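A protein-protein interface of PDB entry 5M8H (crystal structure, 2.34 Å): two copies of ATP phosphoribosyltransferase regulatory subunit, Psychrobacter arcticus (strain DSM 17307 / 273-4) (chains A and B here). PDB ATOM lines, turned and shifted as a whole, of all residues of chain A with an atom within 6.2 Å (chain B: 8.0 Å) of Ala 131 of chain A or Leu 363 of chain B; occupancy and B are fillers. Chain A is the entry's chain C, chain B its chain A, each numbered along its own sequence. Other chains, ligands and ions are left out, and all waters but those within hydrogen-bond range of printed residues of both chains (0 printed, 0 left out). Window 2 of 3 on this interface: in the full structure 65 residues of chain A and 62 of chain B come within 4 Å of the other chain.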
ATOM      1  N   ILE A  94      21.156 -30.603   4.406  1.00  0.00           N
ATOM      2  CA  ILE A  94      21.781 -29.903   5.512  1.00  0.00           C
ATOM      3  C   ILE A  94      21.024 -30.209   6.788  1.00  0.00           C
ATOM      4  O   ILE A  94      19.800 -30.260   6.784  1.00  0.00           O
ATOM      5  CB  ILE A  94      21.843 -28.400   5.253  1.00  0.00           C
ATOM      6  CG1 ILE A  94      22.855 -28.139   4.131  1.00  0.00           C
ATOM      7  CG2 ILE A  94      22.254 -27.641   6.510  1.00  0.00           C
ATOM      8  CD1 ILE A  94      22.693 -26.790   3.451  1.00  0.00           C
ATOM      9  N   ARG A  96      21.376 -29.328  11.213  1.00  0.00           N
ATOM     10  CA  ARG A  96      22.030 -28.584  12.255  1.00  0.00           C
ATOM     11  C   ARG A  96      21.689 -29.180  13.605  1.00  0.00           C
ATOM     12  O   ARG A  96      20.521 -29.503  13.863  1.00  0.00           O
ATOM     13  CB  ARG A  96      21.542 -27.139  12.200  1.00  0.00           C
ATOM     14  CG  ARG A  96      22.001 -26.364  10.964  1.00  0.00           C
ATOM     15  CD  ARG A  96      21.506 -24.947  11.048  1.00  0.00           C
ATOM     16  NE  ARG A  96      21.917 -24.102   9.929  1.00  0.00           N
ATOM     17  CZ  ARG A  96      21.438 -24.166   8.697  1.00  0.00           C
ATOM     18  NH1 ARG A  96      20.531 -25.077   8.374  1.00  0.00           N
ATOM     19  NH2 ARG A  96      21.898 -23.339   7.764  1.00  0.00           N
ATOM     20  N   ILE A 124      27.134 -28.463  11.991  1.00  0.00           N
ATOM     21  CA  ILE A 124      26.399 -28.397  10.725  1.00  0.00           C
ATOM     22  C   ILE A 124      26.872 -29.537   9.855  1.00  0.00           C
ATOM     23  O   ILE A 124      28.066 -29.624   9.557  1.00  0.00           O
ATOM     24  CB  ILE A 124      26.643 -27.093   9.947  1.00  0.00           C
ATOM     25  CG1 ILE A 124      26.225 -25.908  10.802  1.00  0.00           C
ATOM     26  CG2 ILE A 124      25.840 -27.094   8.653  1.00  0.00           C
ATOM     27  CD1 ILE A 124      26.454 -24.568  10.156  1.00  0.00           C
ATOM     28  N   CYS A 127      26.920 -29.722   4.292  1.00  0.00           N
ATOM     29  CA  CYS A 127      27.248 -28.554   3.466  1.00  0.00           C
ATOM     30  C   CYS A 127      28.755 -28.477   3.202  1.00  0.00           C
ATOM     31  O   CYS A 127      29.546 -28.391   4.134  1.00  0.00           O
ATOM     32  CB  CYS A 127      26.772 -27.264   4.127  1.00  0.00           C
ATOM     33  SG  CYS A 127      27.118 -25.772   3.156  1.00  0.00           S
ATOM     34  N   GLU A 128      29.130 -28.460   1.930  1.00  0.00           N
ATOM     35  CA  GLU A 128      30.538 -28.470   1.494  1.00  0.00           C
ATOM     36  C   GLU A 128      31.136 -27.055   1.631  1.00  0.00           C
ATOM     37  O   GLU A 128      32.321 -26.901   1.860  1.00  0.00           O
ATOM     38  CB  GLU A 128      30.712 -28.952   0.035  1.00  0.00           C
ATOM     39  CG  GLU A 128      29.561 -29.809  -0.593  1.00  0.00           C
ATOM     40  CD  GLU A 128      29.985 -30.944  -1.522  1.00  0.00           C
ATOM     41  OE1 GLU A 128      30.651 -30.639  -2.543  1.00  0.00           O
ATOM     42  OE2 GLU A 128      29.588 -32.141  -1.293  1.00  0.00           O
ATOM     43  N   SER A 129      30.297 -26.044   1.460  1.00  0.00           N
ATOM     44  CA  SER A 129      30.744 -24.671   1.363  1.00  0.00           C
ATOM     45  C   SER A 129      31.383 -24.128   2.642  1.00  0.00           C
ATOM     46  O   SER A 129      30.970 -24.446   3.754  1.00  0.00           O
ATOM     47  CB  SER A 129      29.565 -23.775   0.983  1.00  0.00           C
ATOM     48  OG  SER A 129      29.969 -22.413   0.920  1.00  0.00           O
ATOM     49  N   ILE A 130      32.367 -23.266   2.456  1.00  0.00           N
ATOM     50  CA  ILE A 130      32.913 -22.425   3.522  1.00  0.00           C
ATOM     51  C   ILE A 130      31.816 -21.552   4.216  1.00  0.00           C
ATOM     52  O   ILE A 130      32.028 -21.044   5.311  1.00  0.00           O
ATOM     53  CB  ILE A 130      34.070 -21.561   2.957  1.00  0.00           C
ATOM     54  CG1 ILE A 130      34.914 -20.881   4.057  1.00  0.00           C
ATOM     55  CG2 ILE A 130      33.537 -20.506   1.972  1.00  0.00           C
ATOM     56  CD1 ILE A 130      35.615 -21.811   5.012  1.00  0.00           C
ATOM     57  N   ALA A 131      30.665 -21.362   3.559  1.00  0.00           N
ATOM     58  CA  ALA A 131      29.509 -20.684   4.159  1.00  0.00           C
ATOM     59  C   ALA A 131      28.998 -21.318   5.473  1.00  0.00           C
ATOM     60  O   ALA A 131      28.535 -20.598   6.361  1.00  0.00           O
ATOM     61  CB  ALA A 131      28.369 -20.580   3.158  1.00  0.00           C
ATOM     62  N   ALA A 132      29.081 -22.640   5.586  1.00  0.00           N
ATOM     63  CA  ALA A 132      28.724 -23.335   6.839  1.00  0.00           C
ATOM     64  C   ALA A 132      29.660 -22.980   7.994  1.00  0.00           C
ATOM     65  O   ALA A 132      29.227 -22.775   9.115  1.00  0.00           O
ATOM     66  CB  ALA A 132      28.689 -24.837   6.639  1.00  0.00           C
ATOM     67  N   ASP A 133      30.946 -22.914   7.702  1.00  0.00           N
ATOM     68  CA  ASP A 133      31.941 -22.487   8.679  1.00  0.00           C
ATOM     69  C   ASP A 133      31.742 -21.009   9.061  1.00  0.00           C
ATOM     70  O   ASP A 133      31.967 -20.630  10.195  1.00  0.00           O
ATOM     71  CB  ASP A 133      33.348 -22.710   8.153  1.00  0.00           C
ATOM     72  CG  ASP A 133      33.597 -24.176   7.754  1.00  0.00           C
ATOM     73  OD1 ASP A 133      33.919 -25.001   8.636  1.00  0.00           O
ATOM     74  OD2 ASP A 133      33.468 -24.496   6.558  1.00  0.00           O
ATOM     75  N   ILE A 134      31.303 -20.179   8.121  1.00  0.00           N
ATOM     76  CA  ILE A 134      31.019 -18.778   8.406  1.00  0.00           C
ATOM     77  C   ILE A 134      29.768 -18.610   9.290  1.00  0.00           C
ATOM     78  O   ILE A 134      29.719 -17.731  10.163  1.00  0.00           O
ATOM     79  CB  ILE A 134      30.899 -17.977   7.098  1.00  0.00           C
ATOM     80  CG1 ILE A 134      32.277 -17.899   6.444  1.00  0.00           C
ATOM     81  CG2 ILE A 134      30.294 -16.569   7.341  1.00  0.00           C
ATOM     82  CD1 ILE A 134      32.274 -17.345   5.032  1.00  0.00           C
ATOM     83  N   GLU A 135      28.750 -19.444   9.057  1.00  0.00           N
ATOM     84  CA  GLU A 135      27.538 -19.413   9.882  1.00  0.00           C
ATOM     85  C   GLU A 135      27.856 -19.782  11.340  1.00  0.00           C
ATOM     86  O   GLU A 135      27.397 -19.116  12.268  1.00  0.00           O
ATOM     87  CB  GLU A 135      26.486 -20.361   9.348  1.00  0.00           C
ATOM     88  CG  GLU A 135      25.153 -20.262  10.098  1.00  0.00           C
ATOM     89  CD  GLU A 135      24.196 -21.359   9.694  1.00  0.00           C
ATOM     90  OE1 GLU A 135      24.125 -21.678   8.482  1.00  0.00           O
ATOM     91  OE2 GLU A 135      23.523 -21.900  10.585  1.00  0.00           O
ATOM     92  N   LEU A 136      28.652 -20.833  11.511  1.00  0.00           N
ATOM     93  CA  LEU A 136      29.129 -21.246  12.833  1.00  0.00           C
ATOM     94  C   LEU A 136      29.886 -20.160  13.586  1.00  0.00           C
ATOM     95  O   LEU A 136      29.699 -19.982  14.789  1.00  0.00           O
ATOM     96  CB  LEU A 136      29.997 -22.504  12.744  1.00  0.00           C
ATOM     97  CG  LEU A 136      29.208 -23.803  12.656  1.00  0.00           C
ATOM     98  CD1 LEU A 136      30.162 -24.919  12.247  1.00  0.00           C
ATOM     99  CD2 LEU A 136      28.531 -24.150  13.968  1.00  0.00           C
ATOM    100  N   ARG A 288      36.470 -28.418  10.531  1.00  0.00           N
ATOM    101  CA  ARG A 288      35.898 -29.401   9.623  1.00  0.00           C
ATOM    102  C   ARG A 288      36.272 -30.808  10.053  1.00  0.00           C
ATOM    103  O   ARG A 288      37.398 -31.047  10.524  1.00  0.00           O
ATOM    104  CB  ARG A 288      36.434 -29.173   8.219  1.00  0.00           C
ATOM    105  CG  ARG A 288      35.747 -28.064   7.477  1.00  0.00           C
ATOM    106  CD  ARG A 288      34.461 -28.553   6.846  1.00  0.00           C
ATOM    107  NE  ARG A 288      33.650 -27.425   6.419  1.00  0.00           N
ATOM    108  CZ  ARG A 288      32.484 -27.544   5.800  1.00  0.00           C
ATOM    109  NH1 ARG A 288      31.970 -28.733   5.498  1.00  0.00           N
ATOM    110  NH2 ARG A 288      31.842 -26.447   5.451  1.00  0.00           N
ATOM    111  N   LEU B 328      12.286 -19.695   8.041  1.00  0.00           N
ATOM    112  CA  LEU B 328      13.364 -19.735   7.045  1.00  0.00           C
ATOM    113  C   LEU B 328      13.425 -18.434   6.279  1.00  0.00           C
ATOM    114  O   LEU B 328      12.434 -17.966   5.737  1.00  0.00           O
ATOM    115  CB  LEU B 328      13.135 -20.873   6.071  1.00  0.00           C
ATOM    116  CG  LEU B 328      14.067 -20.948   4.877  1.00  0.00           C
ATOM    117  CD1 LEU B 328      15.525 -21.124   5.315  1.00  0.00           C
ATOM    118  CD2 LEU B 328      13.609 -22.106   3.996  1.00  0.00           C
ATOM    119  N   ILE B 329      14.595 -17.836   6.227  1.00  0.00           N
ATOM    120  CA  ILE B 329      14.787 -16.666   5.395  1.00  0.00           C
ATOM    121  C   ILE B 329      14.885 -17.139   3.947  1.00  0.00           C
ATOM    122  O   ILE B 329      15.497 -18.165   3.686  1.00  0.00           O
ATOM    123  CB  ILE B 329      16.022 -15.883   5.844  1.00  0.00           C
ATOM    124  CG1 ILE B 329      15.749 -15.274   7.212  1.00  0.00           C
ATOM    125  CG2 ILE B 329      16.380 -14.799   4.846  1.00  0.00           C
ATOM    126  CD1 ILE B 329      17.002 -14.940   7.964  1.00  0.00           C
ATOM    127  N   TYR B 331      16.246 -17.607   0.459  1.00  0.00           N
ATOM    128  CA  TYR B 331      17.638 -17.643   0.009  1.00  0.00           C
ATOM    129  C   TYR B 331      17.972 -16.567  -1.048  1.00  0.00           C
ATOM    130  O   TYR B 331      18.870 -15.734  -0.853  1.00  0.00           O
ATOM    131  CB  TYR B 331      17.981 -19.068  -0.485  1.00  0.00           C
ATOM    132  CG  TYR B 331      19.396 -19.223  -0.968  1.00  0.00           C
ATOM    133  CD1 TYR B 331      20.463 -19.279  -0.061  1.00  0.00           C
ATOM    134  CD2 TYR B 331      19.683 -19.297  -2.330  1.00  0.00           C
ATOM    135  CE1 TYR B 331      21.766 -19.399  -0.503  1.00  0.00           C
ATOM    136  CE2 TYR B 331      20.984 -19.426  -2.788  1.00  0.00           C
ATOM    137  CZ  TYR B 331      22.019 -19.471  -1.867  1.00  0.00           C
ATOM    138  OH  TYR B 331      23.309 -19.603  -2.292  1.00  0.00           O
ATOM    139  N   ASN B 335      20.403 -13.064  -0.784  1.00  0.00           N
ATOM    140  CA  ASN B 335      21.652 -12.891  -1.538  1.00  0.00           C
ATOM    141  C   ASN B 335      21.638 -11.727  -2.539  1.00  0.00           C
ATOM    142  O   ASN B 335      22.705 -11.274  -2.956  1.00  0.00           O
ATOM    143  CB  ASN B 335      22.062 -14.186  -2.232  1.00  0.00           C
ATOM    144  CG  ASN B 335      22.355 -15.295  -1.256  1.00  0.00           C
ATOM    145  OD1 ASN B 335      23.290 -15.237  -0.449  1.00  0.00           O
ATOM    146  ND2 ASN B 335      21.530 -16.321  -1.310  1.00  0.00           N
ATOM    147  N   THR B 360      16.395 -19.718  10.702  1.00  0.00           N
ATOM    148  CA  THR B 360      17.488 -20.297   9.926  1.00  0.00           C
ATOM    149  C   THR B 360      17.880 -19.342   8.798  1.00  0.00           C
ATOM    150  O   THR B 360      17.027 -18.874   8.037  1.00  0.00           O
ATOM    151  CB  THR B 360      17.062 -21.649   9.321  1.00  0.00           C
ATOM    152  OG1 THR B 360      16.815 -22.582  10.373  1.00  0.00           O
ATOM    153  CG2 THR B 360      18.144 -22.230   8.419  1.00  0.00           C
ATOM    154  N   MET B 361      19.171 -19.056   8.711  1.00  0.00           N
ATOM    155  CA  MET B 361      19.752 -18.309   7.606  1.00  0.00           C
ATOM    156  C   MET B 361      20.290 -19.345   6.629  1.00  0.00           C
ATOM    157  O   MET B 361      21.269 -20.026   6.945  1.00  0.00           O
ATOM    158  CB  MET B 361      20.888 -17.419   8.112  1.00  0.00           C
ATOM    159  CG  MET B 361      21.613 -16.639   7.030  1.00  0.00           C
ATOM    160  SD  MET B 361      20.581 -15.417   6.232  1.00  0.00           S
ATOM    161  CE  MET B 361      20.196 -14.315   7.612  1.00  0.00           C
ATOM    162  N   PRO B 362      19.658 -19.478   5.450  1.00  0.00           N
ATOM    163  CA  PRO B 362      19.946 -20.607   4.546  1.00  0.00           C
ATOM    164  C   PRO B 362      21.311 -20.570   3.914  1.00  0.00           C
ATOM    165  O   PRO B 362      21.753 -19.516   3.521  1.00  0.00           O
ATOM    166  CB  PRO B 362      18.878 -20.478   3.463  1.00  0.00           C
ATOM    167  CG  PRO B 362      18.621 -19.007   3.409  1.00  0.00           C
ATOM    168  CD  PRO B 362      18.684 -18.546   4.847  1.00  0.00           C
ATOM    169  N   LEU B 363      21.974 -21.721   3.858  1.00  0.00           N
ATOM    170  CA  LEU B 363      23.293 -21.868   3.206  1.00  0.00           C
ATOM    171  C   LEU B 363      23.114 -22.078   1.703  1.00  0.00           C
ATOM    172  O   LEU B 363      24.000 -21.764   0.918  1.00  0.00           O
ATOM    173  CB  LEU B 363      24.063 -23.042   3.805  1.00  0.00           C
ATOM    174  CG  LEU B 363      24.459 -22.896   5.272  1.00  0.00           C
ATOM    175  CD1 LEU B 363      24.784 -24.244   5.896  1.00  0.00           C
ATOM    176  CD2 LEU B 363      25.626 -21.950   5.422  1.00  0.00           C
ATOM    177  N   THR B 364      21.969 -22.636   1.323  1.00  0.00           N
ATOM    178  CA  THR B 364      21.620 -22.916  -0.063  1.00  0.00           C
ATOM    179  C   THR B 364      20.123 -22.742  -0.252  1.00  0.00           C
ATOM    180  O   THR B 364      19.350 -22.645   0.721  1.00  0.00           O
ATOM    181  CB  THR B 364      21.938 -24.375  -0.461  1.00  0.00           C
ATOM    182  OG1 THR B 364      21.012 -25.271   0.182  1.00  0.00           O
ATOM    183  CG2 THR B 364      23.393 -24.746  -0.137  1.00  0.00           C
ATOM    184  N   ALA B 365      19.718 -22.766  -1.517  1.00  0.00           N
ATOM    185  CA  ALA B 365      18.310 -22.705  -1.890  1.00  0.00           C
ATOM    186  C   ALA B 365      17.506 -23.915  -1.433  1.00  0.00           C
ATOM    187  O   ALA B 365      16.301 -23.811  -1.322  1.00  0.00           O
ATOM    188  CB  ALA B 365      18.189 -22.557  -3.400  1.00  0.00           C
ATOM    189  N   GLU B 366      18.152 -25.045  -1.163  1.00  0.00           N
ATOM    190  CA  GLU B 366      17.464 -26.271  -0.679  1.00  0.00           C
ATOM    191  C   GLU B 366      17.449 -26.386   0.857  1.00  0.00           C
ATOM    192  O   GLU B 366      16.788 -27.258   1.385  1.00  0.00           O
ATOM    193  CB  GLU B 366      18.001 -27.589  -1.326  1.00  0.00           C
ATOM    194  CG  GLU B 366      19.214 -27.567  -2.296  1.00  0.00           C
ATOM    195  CD  GLU B 366      19.026 -26.645  -3.490  1.00  0.00           C
ATOM    196  OE1 GLU B 366      17.893 -26.549  -4.032  1.00  0.00           O
ATOM    197  OE2 GLU B 366      20.035 -25.998  -3.872  1.00  0.00           O
ATOM    198  N   ASP B 367      18.158 -25.492   1.549  1.00  0.00           N
ATOM    199  CA  ASP B 367      18.269 -25.495   3.011  1.00  0.00           C
ATOM    200  C   ASP B 367      16.900 -25.262   3.658  1.00  0.00           C
ATOM    201  O   ASP B 367      16.330 -24.172   3.604  1.00  0.00           O
ATOM    202  CB  ASP B 367      19.273 -24.404   3.447  1.00  0.00           C
ATOM    203  CG  ASP B 367      19.741 -24.537   4.894  1.00  0.00           C
ATOM    204  OD1 ASP B 367      19.215 -25.327   5.670  1.00  0.00           O
ATOM    205  OD2 ASP B 367      20.689 -23.813   5.247  1.00  0.00           O
ATOM    206  N   MET B 368      16.398 -26.313   4.285  1.00  0.00           N
ATOM    207  CA  MET B 368      15.013 -26.399   4.723  1.00  0.00           C
ATOM    208  C   MET B 368      15.014 -26.861   6.188  1.00  0.00           C
ATOM    209  O   MET B 368      15.357 -28.015   6.474  1.00  0.00           O
ATOM    210  CB  MET B 368      14.292 -27.440   3.857  1.00  0.00           C
ATOM    211  CG  MET B 368      12.813 -27.629   4.124  1.00  0.00           C
ATOM    212  SD  MET B 368      11.847 -26.128   3.919  1.00  0.00           S
ATOM    213  CE  MET B 368      12.261 -25.593   2.244  1.00  0.00           C
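CD1 of Ile 94 of chain A touches OG1 of Thr 364 of chain B, 3.98 Å away.
Asp 367 of chain B touches Ile 94 of chain A (OD1 to CG2, 3.9 Å).
Arg 96 of chain A touches Thr 360 of chain B.
Arg 96 of chain A touches Leu 363 of chain B (NH2 to CD1, 3.6 Å).
Cys 127 of chain A touches Leu 363 of chain B.
O of Ala 131 of chain A touches CD2 of Leu 363 of chain B, at 3.3 Å.
Ala 132 of chain A touches Leu 363 of chain B (N to CD2, 3.5 Å).
O of Met 361 of chain B touches OE1 of Glu 135 of chain A, at 3.6 Å.
OE1 of Glu 135 of chain A touches CD2 of Leu 363 of chain B, 3.4 Å away.
SG of Cys 127 of chain A lies close to N of Ser 129 of chain A.
OG1 of Thr 364 of chain B sits close to N of Glu 366 of chain B, at 3.2 Å.
The guanidinium group (NE) of Arg 96 of chain A lies within salt-bridge range of the side-chain carboxylate (OE2) of Glu 135 of chain A, 2.8 Å away.
O of Thr 360 of chain B lies within hydrogen-bond range of N of Ile 329 of chain B (3.2 Å).
The side-chain hydroxyl (OG) of Ser 129 of chain A sits at hydrogen-bond distance from the backbone NH (N) of Ala 131 of chain A (2.9 Å).
The side-chain hydroxyl (OG1) of Thr 364 of chain B is in hydrogen-bond range of the backbone NH (N) of Asp 367 of chain B (3.2 Å).
The side-chain carboxylate of Asp 367 of chain B lies within salt-bridge range of the guanidinium group of Arg 96 of chain A.
The guanidinium group (NH2) of Arg 96 of chain A lies within hydrogen-bond range of the backbone carbonyl oxygen (O) of Met 361 of chain B (3.5 Å).
Of chain B, only Leu 363 (3.3 Å) comes within 4 Å of Ala 131 of chain A.
Of the printed residues of chain A, Leu 363 of chain B touches Arg 96, Cys 127, Ala 131, Ala 132 and Glu 135.
Of chain B, only Leu 363 comes within 4 Å of Ala 132 of chain A.
Of the printed residues of chain A, Asp 367 of chain B touches Ile 94 and Arg 96.
Printed residues of chain B within 4 Å of Ile 94 of chain A: Thr 364 and Asp 367.
Printed residues of chain B within 4 Å of Cys 127 of chain A: Leu 363.
Printed residues of chain A within 4 Å of Met 361 of chain B: Arg 96 and Glu 135.
Ser 129 of chain A touches none of the printed residues of chain B.
The nearest printed residue of chain A that does not touch Leu 363 of chain B is Ile 94 of chain A (4.01 Å).
The nearest printed residue of chain A that does not touch Asp 367 of chain B is Glu 135 of chain A (5.2 Å).
No position is printed for both chains.
Of the 11 pairs that touch across the chains among the printed residues, none has its exchanged pair printed and touching as well.
Of the 13 printed residues of chain B, 5 touch a printed residue of chain A.
Among the printed residues, 11 pairs touch across the chains.
Among the printed residues, Asp or Glu carboxylates within 4 Å of a Lys or Arg side-chain nitrogen of the other chain: Arg 96 of chain A with Asp 367 of chain B (2.8 Å).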
